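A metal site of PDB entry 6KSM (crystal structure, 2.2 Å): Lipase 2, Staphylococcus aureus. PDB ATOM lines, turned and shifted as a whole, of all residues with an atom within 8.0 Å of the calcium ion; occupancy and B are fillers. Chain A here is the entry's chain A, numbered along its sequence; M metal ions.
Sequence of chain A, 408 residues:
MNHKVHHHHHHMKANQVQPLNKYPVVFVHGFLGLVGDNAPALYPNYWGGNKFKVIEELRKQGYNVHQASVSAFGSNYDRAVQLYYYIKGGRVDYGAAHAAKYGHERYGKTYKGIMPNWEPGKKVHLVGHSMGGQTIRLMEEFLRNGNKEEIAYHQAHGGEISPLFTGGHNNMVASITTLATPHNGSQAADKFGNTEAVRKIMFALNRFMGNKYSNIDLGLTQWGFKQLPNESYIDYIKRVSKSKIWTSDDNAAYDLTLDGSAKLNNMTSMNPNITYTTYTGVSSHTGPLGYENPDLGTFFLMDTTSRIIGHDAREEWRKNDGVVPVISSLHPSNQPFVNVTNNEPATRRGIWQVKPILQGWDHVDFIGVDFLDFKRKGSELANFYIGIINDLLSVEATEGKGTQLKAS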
ATOM      1  N   LYS A  51     -10.580 -18.146   9.483  1.00  0.00           N
ATOM      2  CA  LYS A  51     -11.103 -18.923   8.369  1.00  0.00           C
ATOM      3  C   LYS A  51     -12.480 -18.433   7.975  1.00  0.00           C
ATOM      4  O   LYS A  51     -12.753 -18.189   6.825  1.00  0.00           O
ATOM      5  CB  LYS A  51     -11.069 -20.403   8.691  1.00  0.00           C
ATOM      6  CG  LYS A  51      -9.637 -20.916   8.680  1.00  0.00           C
ATOM      7  CD  LYS A  51      -9.532 -22.390   9.005  1.00  0.00           C
ATOM      8  CE  LYS A  51      -8.082 -22.783   8.807  1.00  0.00           C
ATOM      9  NZ  LYS A  51      -8.022 -24.278   8.796  1.00  0.00           N
ATOM     10  N   SER A 283     -10.611 -37.591  14.257  1.00  0.00           N
ATOM     11  CA  SER A 283      -9.361 -37.203  13.716  1.00  0.00           C
ATOM     12  C   SER A 283      -8.315 -38.199  14.158  1.00  0.00           C
ATOM     13  O   SER A 283      -7.067 -37.890  14.320  1.00  0.00           O
ATOM     14  CB  SER A 283      -9.076 -35.722  14.180  1.00  0.00           C
ATOM     15  OG  SER A 283      -7.852 -35.305  13.578  1.00  0.00           O
ATOM     16  N   ASP A 295      -4.624 -38.459  13.446  1.00  0.00           N
ATOM     17  CA  ASP A 295      -4.293 -38.149  12.036  1.00  0.00           C
ATOM     18  C   ASP A 295      -3.280 -37.020  11.979  1.00  0.00           C
ATOM     19  O   ASP A 295      -3.263 -36.136  12.874  1.00  0.00           O
ATOM     20  CB  ASP A 295      -5.560 -37.627  11.310  1.00  0.00           C
ATOM     21  CG  ASP A 295      -6.690 -38.675  11.212  1.00  0.00           C
ATOM     22  OD1 ASP A 295      -6.518 -39.876  11.650  1.00  0.00           O
ATOM     23  OD2 ASP A 295      -7.747 -38.266  10.674  1.00  0.00           O
ATOM     24  N   LEU A 296      -2.426 -37.043  10.950  1.00  0.00           N
ATOM     25  CA  LEU A 296      -1.675 -35.876  10.516  1.00  0.00           C
ATOM     26  C   LEU A 296      -2.657 -34.704  10.388  1.00  0.00           C
ATOM     27  O   LEU A 296      -3.808 -34.856   9.869  1.00  0.00           O
ATOM     28  CB  LEU A 296      -1.033 -36.169   9.180  1.00  0.00           C
ATOM     29  CG  LEU A 296       0.424 -36.657   9.134  1.00  0.00           C
ATOM     30  CD1 LEU A 296       0.901 -37.487  10.355  1.00  0.00           C
ATOM     31  CD2 LEU A 296       0.634 -37.384   7.801  1.00  0.00           C
ATOM     32  N   GLY A 297      -2.259 -33.568  10.935  1.00  0.00           N
ATOM     33  CA  GLY A 297      -3.159 -32.437  10.843  1.00  0.00           C
ATOM     34  C   GLY A 297      -4.291 -32.330  11.853  1.00  0.00           C
ATOM     35  O   GLY A 297      -5.192 -31.429  11.720  1.00  0.00           O
ATOM     36  N   THR A 298      -4.259 -33.237  12.849  1.00  0.00           N
ATOM     37  CA  THR A 298      -4.853 -32.922  14.130  1.00  0.00           C
ATOM     38  C   THR A 298      -4.042 -31.727  14.686  1.00  0.00           C
ATOM     39  O   THR A 298      -2.770 -31.770  14.739  1.00  0.00           O
ATOM     40  CB  THR A 298      -4.672 -34.098  15.138  1.00  0.00           C
ATOM     41  OG1 THR A 298      -5.137 -35.319  14.552  1.00  0.00           O
ATOM     42  CG2 THR A 298      -5.400 -33.834  16.485  1.00  0.00           C
ATOM     43  N   PHE A 299      -4.724 -30.667  15.090  1.00  0.00           N
ATOM     44  CA  PHE A 299      -4.031 -29.580  15.735  1.00  0.00           C
ATOM     45  C   PHE A 299      -2.993 -30.111  16.747  1.00  0.00           C
ATOM     46  O   PHE A 299      -3.317 -30.888  17.630  1.00  0.00           O
ATOM     47  CB  PHE A 299      -4.974 -28.559  16.346  1.00  0.00           C
ATOM     48  CG  PHE A 299      -4.257 -27.285  16.727  1.00  0.00           C
ATOM     49  CD1 PHE A 299      -3.581 -26.521  15.729  1.00  0.00           C
ATOM     50  CD2 PHE A 299      -4.193 -26.877  18.051  1.00  0.00           C
ATOM     51  CE1 PHE A 299      -2.875 -25.361  16.063  1.00  0.00           C
ATOM     52  CE2 PHE A 299      -3.479 -25.735  18.396  1.00  0.00           C
ATOM     53  CZ  PHE A 299      -2.814 -24.979  17.402  1.00  0.00           C
ATOM     54  N   PHE A 300      -1.725 -29.749  16.578  1.00  0.00           N
ATOM     55  CA  PHE A 300      -0.627 -30.447  17.279  1.00  0.00           C
ATOM     56  C   PHE A 300      -0.660 -30.368  18.840  1.00  0.00           C
ATOM     57  O   PHE A 300      -0.113 -31.250  19.524  1.00  0.00           O
ATOM     58  CB  PHE A 300       0.748 -29.939  16.779  1.00  0.00           C
ATOM     59  CG  PHE A 300       1.145 -28.561  17.333  1.00  0.00           C
ATOM     60  CD1 PHE A 300       0.582 -27.384  16.787  1.00  0.00           C
ATOM     61  CD2 PHE A 300       2.019 -28.447  18.420  1.00  0.00           C
ATOM     62  CE1 PHE A 300       0.916 -26.095  17.308  1.00  0.00           C
ATOM     63  CE2 PHE A 300       2.383 -27.160  18.915  1.00  0.00           C
ATOM     64  CZ  PHE A 300       1.814 -26.001  18.363  1.00  0.00           C
ATOM     65  N   MET A 302      -2.931 -31.222  20.461  1.00  0.00           N
ATOM     66  CA  MET A 302      -3.680 -32.386  20.882  1.00  0.00           C
ATOM     67  C   MET A 302      -3.030 -33.769  20.621  1.00  0.00           C
ATOM     68  O   MET A 302      -3.712 -34.738  20.949  1.00  0.00           O
ATOM     69  CB  MET A 302      -5.131 -32.308  20.365  1.00  0.00           C
ATOM     70  CG  MET A 302      -5.825 -31.037  20.751  1.00  0.00           C
ATOM     71  SD  MET A 302      -7.522 -30.835  20.157  1.00  0.00           S
ATOM     72  CE  MET A 302      -7.411 -30.467  18.432  1.00  0.00           C
ATOM     73  N   ASP A 321     -11.521 -36.714  18.615  1.00  0.00           N
ATOM     74  CA  ASP A 321     -11.321 -35.532  17.782  1.00  0.00           C
ATOM     75  C   ASP A 321     -10.037 -34.803  18.219  1.00  0.00           C
ATOM     76  O   ASP A 321      -9.830 -33.591  17.876  1.00  0.00           O
ATOM     77  CB  ASP A 321     -12.561 -34.622  17.794  1.00  0.00           C
ATOM     78  CG  ASP A 321     -12.705 -33.879  19.139  1.00  0.00           C
ATOM     79  OD1 ASP A 321     -11.801 -34.087  20.017  1.00  0.00           O
ATOM     80  OD2 ASP A 321     -13.670 -33.051  19.304  1.00  0.00           O
ATOM     81  N   GLY A 360     -12.228 -36.344   9.615  1.00  0.00           N
ATOM     82  CA  GLY A 360     -11.044 -35.509   9.521  1.00  0.00           C
ATOM     83  C   GLY A 360     -11.104 -34.189  10.319  1.00  0.00           C
ATOM     84  O   GLY A 360     -10.128 -33.463  10.317  1.00  0.00           O
ATOM     85  N   TRP A 361     -12.243 -33.859  10.953  1.00  0.00           N
ATOM     86  CA  TRP A 361     -12.382 -32.631  11.715  1.00  0.00           C
ATOM     87  C   TRP A 361     -11.900 -32.902  13.164  1.00  0.00           C
ATOM     88  O   TRP A 361     -12.524 -33.729  13.848  1.00  0.00           O
ATOM     89  CB  TRP A 361     -13.818 -32.150  11.725  1.00  0.00           C
ATOM     90  CG  TRP A 361     -14.325 -31.586  10.464  1.00  0.00           C
ATOM     91  CD1 TRP A 361     -14.118 -32.093   9.213  1.00  0.00           C
ATOM     92  CD2 TRP A 361     -15.143 -30.403  10.293  1.00  0.00           C
ATOM     93  NE1 TRP A 361     -14.712 -31.254   8.268  1.00  0.00           N
ATOM     94  CE2 TRP A 361     -15.380 -30.240   8.905  1.00  0.00           C
ATOM     95  CE3 TRP A 361     -15.674 -29.430  11.180  1.00  0.00           C
ATOM     96  CZ2 TRP A 361     -16.147 -29.168   8.363  1.00  0.00           C
ATOM     97  CZ3 TRP A 361     -16.462 -28.353  10.645  1.00  0.00           C
ATOM     98  CH2 TRP A 361     -16.671 -28.240   9.246  1.00  0.00           C
ATOM     99  N   ASP A 362     -10.811 -32.227  13.642  1.00  0.00           N
ATOM    100  CA  ASP A 362     -10.412 -32.337  15.029  1.00  0.00           C
ATOM    101  C   ASP A 362     -11.302 -31.346  15.779  1.00  0.00           C
ATOM    102  O   ASP A 362     -12.121 -30.563  15.159  1.00  0.00           O
ATOM    103  CB  ASP A 362      -8.919 -32.136  15.251  1.00  0.00           C
ATOM    104  CG  ASP A 362      -8.431 -30.741  14.816  1.00  0.00           C
ATOM    105  OD1 ASP A 362      -9.192 -29.725  14.998  1.00  0.00           O
ATOM    106  OD2 ASP A 362      -7.289 -30.669  14.241  1.00  0.00           O
ATOM    107  N   HIS A 363     -11.166 -31.397  17.105  1.00  0.00           N
ATOM    108  CA  HIS A 363     -11.943 -30.540  18.010  1.00  0.00           C
ATOM    109  C   HIS A 363     -12.016 -29.048  17.627  1.00  0.00           C
ATOM    110  O   HIS A 363     -13.084 -28.383  17.689  1.00  0.00           O
ATOM    111  CB  HIS A 363     -11.303 -30.673  19.369  1.00  0.00           C
ATOM    112  CG  HIS A 363     -12.128 -30.058  20.423  1.00  0.00           C
ATOM    113  ND1 HIS A 363     -13.291 -30.647  20.868  1.00  0.00           N
ATOM    114  CD2 HIS A 363     -12.005 -28.886  21.063  1.00  0.00           C
ATOM    115  CE1 HIS A 363     -13.856 -29.829  21.760  1.00  0.00           C
ATOM    116  NE2 HIS A 363     -13.072 -28.775  21.919  1.00  0.00           N
ATOM    117  N   VAL A 364     -10.875 -28.541  17.149  1.00  0.00           N
ATOM    118  CA  VAL A 364     -10.706 -27.115  16.942  1.00  0.00           C
ATOM    119  C   VAL A 364     -10.980 -26.794  15.451  1.00  0.00           C
ATOM    120  O   VAL A 364     -11.187 -25.600  15.110  1.00  0.00           O
ATOM    121  CB  VAL A 364      -9.319 -26.813  17.488  1.00  0.00           C
ATOM    122  CG1 VAL A 364      -8.279 -26.537  16.461  1.00  0.00           C
ATOM    123  CG2 VAL A 364      -9.292 -26.116  18.820  1.00  0.00           C
ATOM    124  N   ASP A 365     -11.084 -27.831  14.577  1.00  0.00           N
ATOM    125  CA  ASP A 365     -11.522 -27.541  13.191  1.00  0.00           C
ATOM    126  C   ASP A 365     -12.907 -26.963  13.189  1.00  0.00           C
ATOM    127  O   ASP A 365     -13.280 -26.195  12.318  1.00  0.00           O
ATOM    128  CB  ASP A 365     -11.394 -28.710  12.258  1.00  0.00           C
ATOM    129  CG  ASP A 365      -9.893 -29.152  12.017  1.00  0.00           C
ATOM    130  OD1 ASP A 365      -8.986 -28.337  11.882  1.00  0.00           O
ATOM    131  OD2 ASP A 365      -9.589 -30.333  11.967  1.00  0.00           O
ATOM    132  N   PHE A 366     -13.679 -27.269  14.219  1.00  0.00           N
ATOM    133  CA  PHE A 366     -15.047 -26.781  14.305  1.00  0.00           C
ATOM    134  C   PHE A 366     -15.139 -25.280  14.506  1.00  0.00           C
ATOM    135  O   PHE A 366     -16.200 -24.700  14.236  1.00  0.00           O
ATOM    136  CB  PHE A 366     -15.772 -27.481  15.470  1.00  0.00           C
ATOM    137  CG  PHE A 366     -16.307 -28.812  15.133  1.00  0.00           C
ATOM    138  CD1 PHE A 366     -17.526 -28.934  14.458  1.00  0.00           C
ATOM    139  CD2 PHE A 366     -15.593 -29.999  15.503  1.00  0.00           C
ATOM    140  CE1 PHE A 366     -18.032 -30.247  14.137  1.00  0.00           C
ATOM    141  CE2 PHE A 366     -16.079 -31.299  15.189  1.00  0.00           C
ATOM    142  CZ  PHE A 366     -17.306 -31.420  14.520  1.00  0.00           C
ATOM    143  N   VAL A 369      -9.733 -22.467  14.329  1.00  0.00           N
ATOM    144  CA  VAL A 369      -8.498 -21.908  14.800  1.00  0.00           C
ATOM    145  C   VAL A 369      -7.294 -22.776  14.456  1.00  0.00           C
ATOM    146  O   VAL A 369      -6.192 -22.361  14.761  1.00  0.00           O
ATOM    147  CB  VAL A 369      -8.498 -21.577  16.332  1.00  0.00           C
ATOM    148  CG1 VAL A 369      -9.724 -20.746  16.715  1.00  0.00           C
ATOM    149  CG2 VAL A 369      -8.476 -22.851  17.167  1.00  0.00           C
ATOM    150  N   ASP A 370      -7.448 -23.989  13.875  1.00  0.00           N
ATOM    151  CA  ASP A 370      -6.257 -24.739  13.384  1.00  0.00           C
ATOM    152  C   ASP A 370      -5.692 -24.088  12.134  1.00  0.00           C
ATOM    153  O   ASP A 370      -5.959 -24.581  11.027  1.00  0.00           O
ATOM    154  CB  ASP A 370      -6.574 -26.195  13.018  1.00  0.00           C
ATOM    155  CG  ASP A 370      -5.286 -27.049  12.813  1.00  0.00           C
ATOM    156  OD1 ASP A 370      -4.202 -26.521  12.541  1.00  0.00           O
ATOM    157  OD2 ASP A 370      -5.324 -28.267  12.984  1.00  0.00           O
ATOM    158  N   PHE A 371      -4.874 -23.044  12.287  1.00  0.00           N
ATOM    159  CA  PHE A 371      -4.292 -22.304  11.124  1.00  0.00           C
ATOM    160  C   PHE A 371      -3.290 -23.214  10.373  1.00  0.00           C
ATOM    161  O   PHE A 371      -3.074 -22.997   9.174  1.00  0.00           O
ATOM    162  CB  PHE A 371      -3.592 -20.946  11.570  1.00  0.00           C
ATOM    163  CG  PHE A 371      -2.494 -21.170  12.593  1.00  0.00           C
ATOM    164  CD1 PHE A 371      -2.816 -21.379  13.957  1.00  0.00           C
ATOM    165  CD2 PHE A 371      -1.140 -21.329  12.188  1.00  0.00           C
ATOM    166  CE1 PHE A 371      -1.815 -21.664  14.936  1.00  0.00           C
ATOM    167  CE2 PHE A 371      -0.135 -21.624  13.158  1.00  0.00           C
ATOM    168  CZ  PHE A 371      -0.471 -21.787  14.533  1.00  0.00           C
ATOM    169  N   LEU A 372      -2.653 -24.179  11.075  1.00  0.00           N
ATOM    170  CA  LEU A 372      -1.774 -25.213  10.437  1.00  0.00           C
ATOM    171  C   LEU A 372      -2.428 -26.195   9.420  1.00  0.00           C
ATOM    172  O   LEU A 372      -1.709 -26.868   8.735  1.00  0.00           O
ATOM    173  CB  LEU A 372      -1.051 -26.083  11.472  1.00  0.00           C
ATOM    174  CG  LEU A 372       0.176 -25.610  12.185  1.00  0.00           C
ATOM    175  CD1 LEU A 372       0.781 -24.407  11.491  1.00  0.00           C
ATOM    176  CD2 LEU A 372      -0.074 -25.271  13.627  1.00  0.00           C
ATOM    177  N   ASP A 373      -3.760 -26.279   9.310  1.00  0.00           N
ATOM    178  CA  ASP A 373      -4.394 -27.395   8.584  1.00  0.00           C
ATOM    179  C   ASP A 373      -5.094 -26.905   7.323  1.00  0.00           C
ATOM    180  O   ASP A 373      -6.241 -26.412   7.387  1.00  0.00           O
ATOM    181  CB  ASP A 373      -5.362 -28.156   9.523  1.00  0.00           C
ATOM    182  CG  ASP A 373      -6.064 -29.472   8.874  1.00  0.00           C
ATOM    183  OD1 ASP A 373      -5.789 -29.887   7.709  1.00  0.00           O
ATOM    184  OD2 ASP A 373      -6.904 -30.084   9.583  1.00  0.00           O
ATOM    185  N   PHE A 374      -4.412 -27.054   6.186  1.00  0.00           N
ATOM    186  CA  PHE A 374      -4.907 -26.459   4.920  1.00  0.00           C
ATOM    187  C   PHE A 374      -6.057 -27.191   4.271  1.00  0.00           C
ATOM    188  O   PHE A 374      -6.673 -26.631   3.387  1.00  0.00           O
ATOM    189  CB  PHE A 374      -3.793 -26.147   3.869  1.00  0.00           C
ATOM    190  CG  PHE A 374      -2.744 -25.193   4.352  1.00  0.00           C
ATOM    191  CD1 PHE A 374      -3.010 -24.208   5.356  1.00  0.00           C
ATOM    192  CD2 PHE A 374      -1.442 -25.237   3.787  1.00  0.00           C
ATOM    193  CE1 PHE A 374      -2.028 -23.316   5.799  1.00  0.00           C
ATOM    194  CE2 PHE A 374      -0.454 -24.346   4.223  1.00  0.00           C
ATOM    195  CZ  PHE A 374      -0.753 -23.392   5.223  1.00  0.00           C
ATOM    196  N   LYS A 375      -6.370 -28.417   4.708  1.00  0.00           N
ATOM    197  CA  LYS A 375      -7.565 -29.197   4.225  1.00  0.00           C
ATOM    198  C   LYS A 375      -8.895 -28.561   4.674  1.00  0.00           C
ATOM    199  O   LYS A 375      -9.938 -28.635   3.998  1.00  0.00           O
ATOM    200  CB  LYS A 375      -7.520 -30.680   4.680  1.00  0.00           C
ATOM    201  CG  LYS A 375      -6.390 -31.541   4.085  1.00  0.00           C
ATOM    202  CD  LYS A 375      -6.282 -32.921   4.739  1.00  0.00           C
ATOM    203  CE  LYS A 375      -5.423 -32.896   6.014  1.00  0.00           C
ATOM    204  NZ  LYS A 375      -6.285 -32.942   7.237  1.00  0.00           N
ATOM    205  N   ARG A 376      -8.875 -27.958   5.854  1.00  0.00           N
ATOM    206  CA  ARG A 376     -10.095 -27.342   6.416  1.00  0.00           C
ATOM    207  C   ARG A 376     -10.101 -25.878   5.974  1.00  0.00           C
ATOM    208  O   ARG A 376      -9.377 -25.061   6.526  1.00  0.00           O
ATOM    209  CB  ARG A 376     -10.164 -27.529   7.944  1.00  0.00           C
ATOM    210  CG  ARG A 376      -9.794 -28.945   8.415  1.00  0.00           C
ATOM    211  CD  ARG A 376     -11.031 -29.853   8.622  1.00  0.00           C
ATOM    212  NE  ARG A 376     -11.862 -30.082   7.428  1.00  0.00           N
ATOM    213  CZ  ARG A 376     -11.649 -31.061   6.499  1.00  0.00           C
ATOM    214  NH1 ARG A 376     -12.497 -31.204   5.474  1.00  0.00           N
ATOM    215  NH2 ARG A 376     -10.621 -31.887   6.572  1.00  0.00           N
HETATM  216 CA    CA M   1      -7.153 -30.120  12.060  1.00  0.00          CA
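O of Asp 373 is in hydrogen-bond range of NZ of Lys 51 (3.1 Å). The backbone carbonyl oxygen of Asp 370 lies within hydrogen-bond range of the side-chain amino group of Lys 51, 3.1 Å away. The side-chain carboxylate (OD1) of Asp 373 lies within salt-bridge range of the side-chain amino group (NZ) of Lys 375. The backbone NH (N) of Val 364 is in hydrogen-bond range of the side-chain carboxylate (OD1) of Asp 362. The side-chain carboxylate (OD2) of Asp 362 lies close to the backbone NH (N) of Phe 299 (2.7 Å). OD2 of Asp 370 sits close to N of Phe 299 (3.2 Å). The side-chain carboxylate (OD1) of Asp 370 is in hydrogen-bond range of the backbone NH (N) of Leu 372, 3.2 Å away.
OD2 of Asp 362 is bound to the calcium ion. The calcium ion is bound by O of Gly 297, 2.4 Å away. The calcium ion is bound by OD2 of Asp 365, at 2.4 Å. The calcium ion is bound by OD2 of Asp 373, 2.5 Å away. OD1 of Asp 365 is bound to the calcium ion, 2.6 Å away. The side-chain carboxylate (OD2) of Asp 370 binds the calcium ion, 2.8 Å away.
N of Phe 299 touches the calcium ion (3.9 Å). Of the 25 residues printed, 6 come within 4 Å of the calcium ion.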
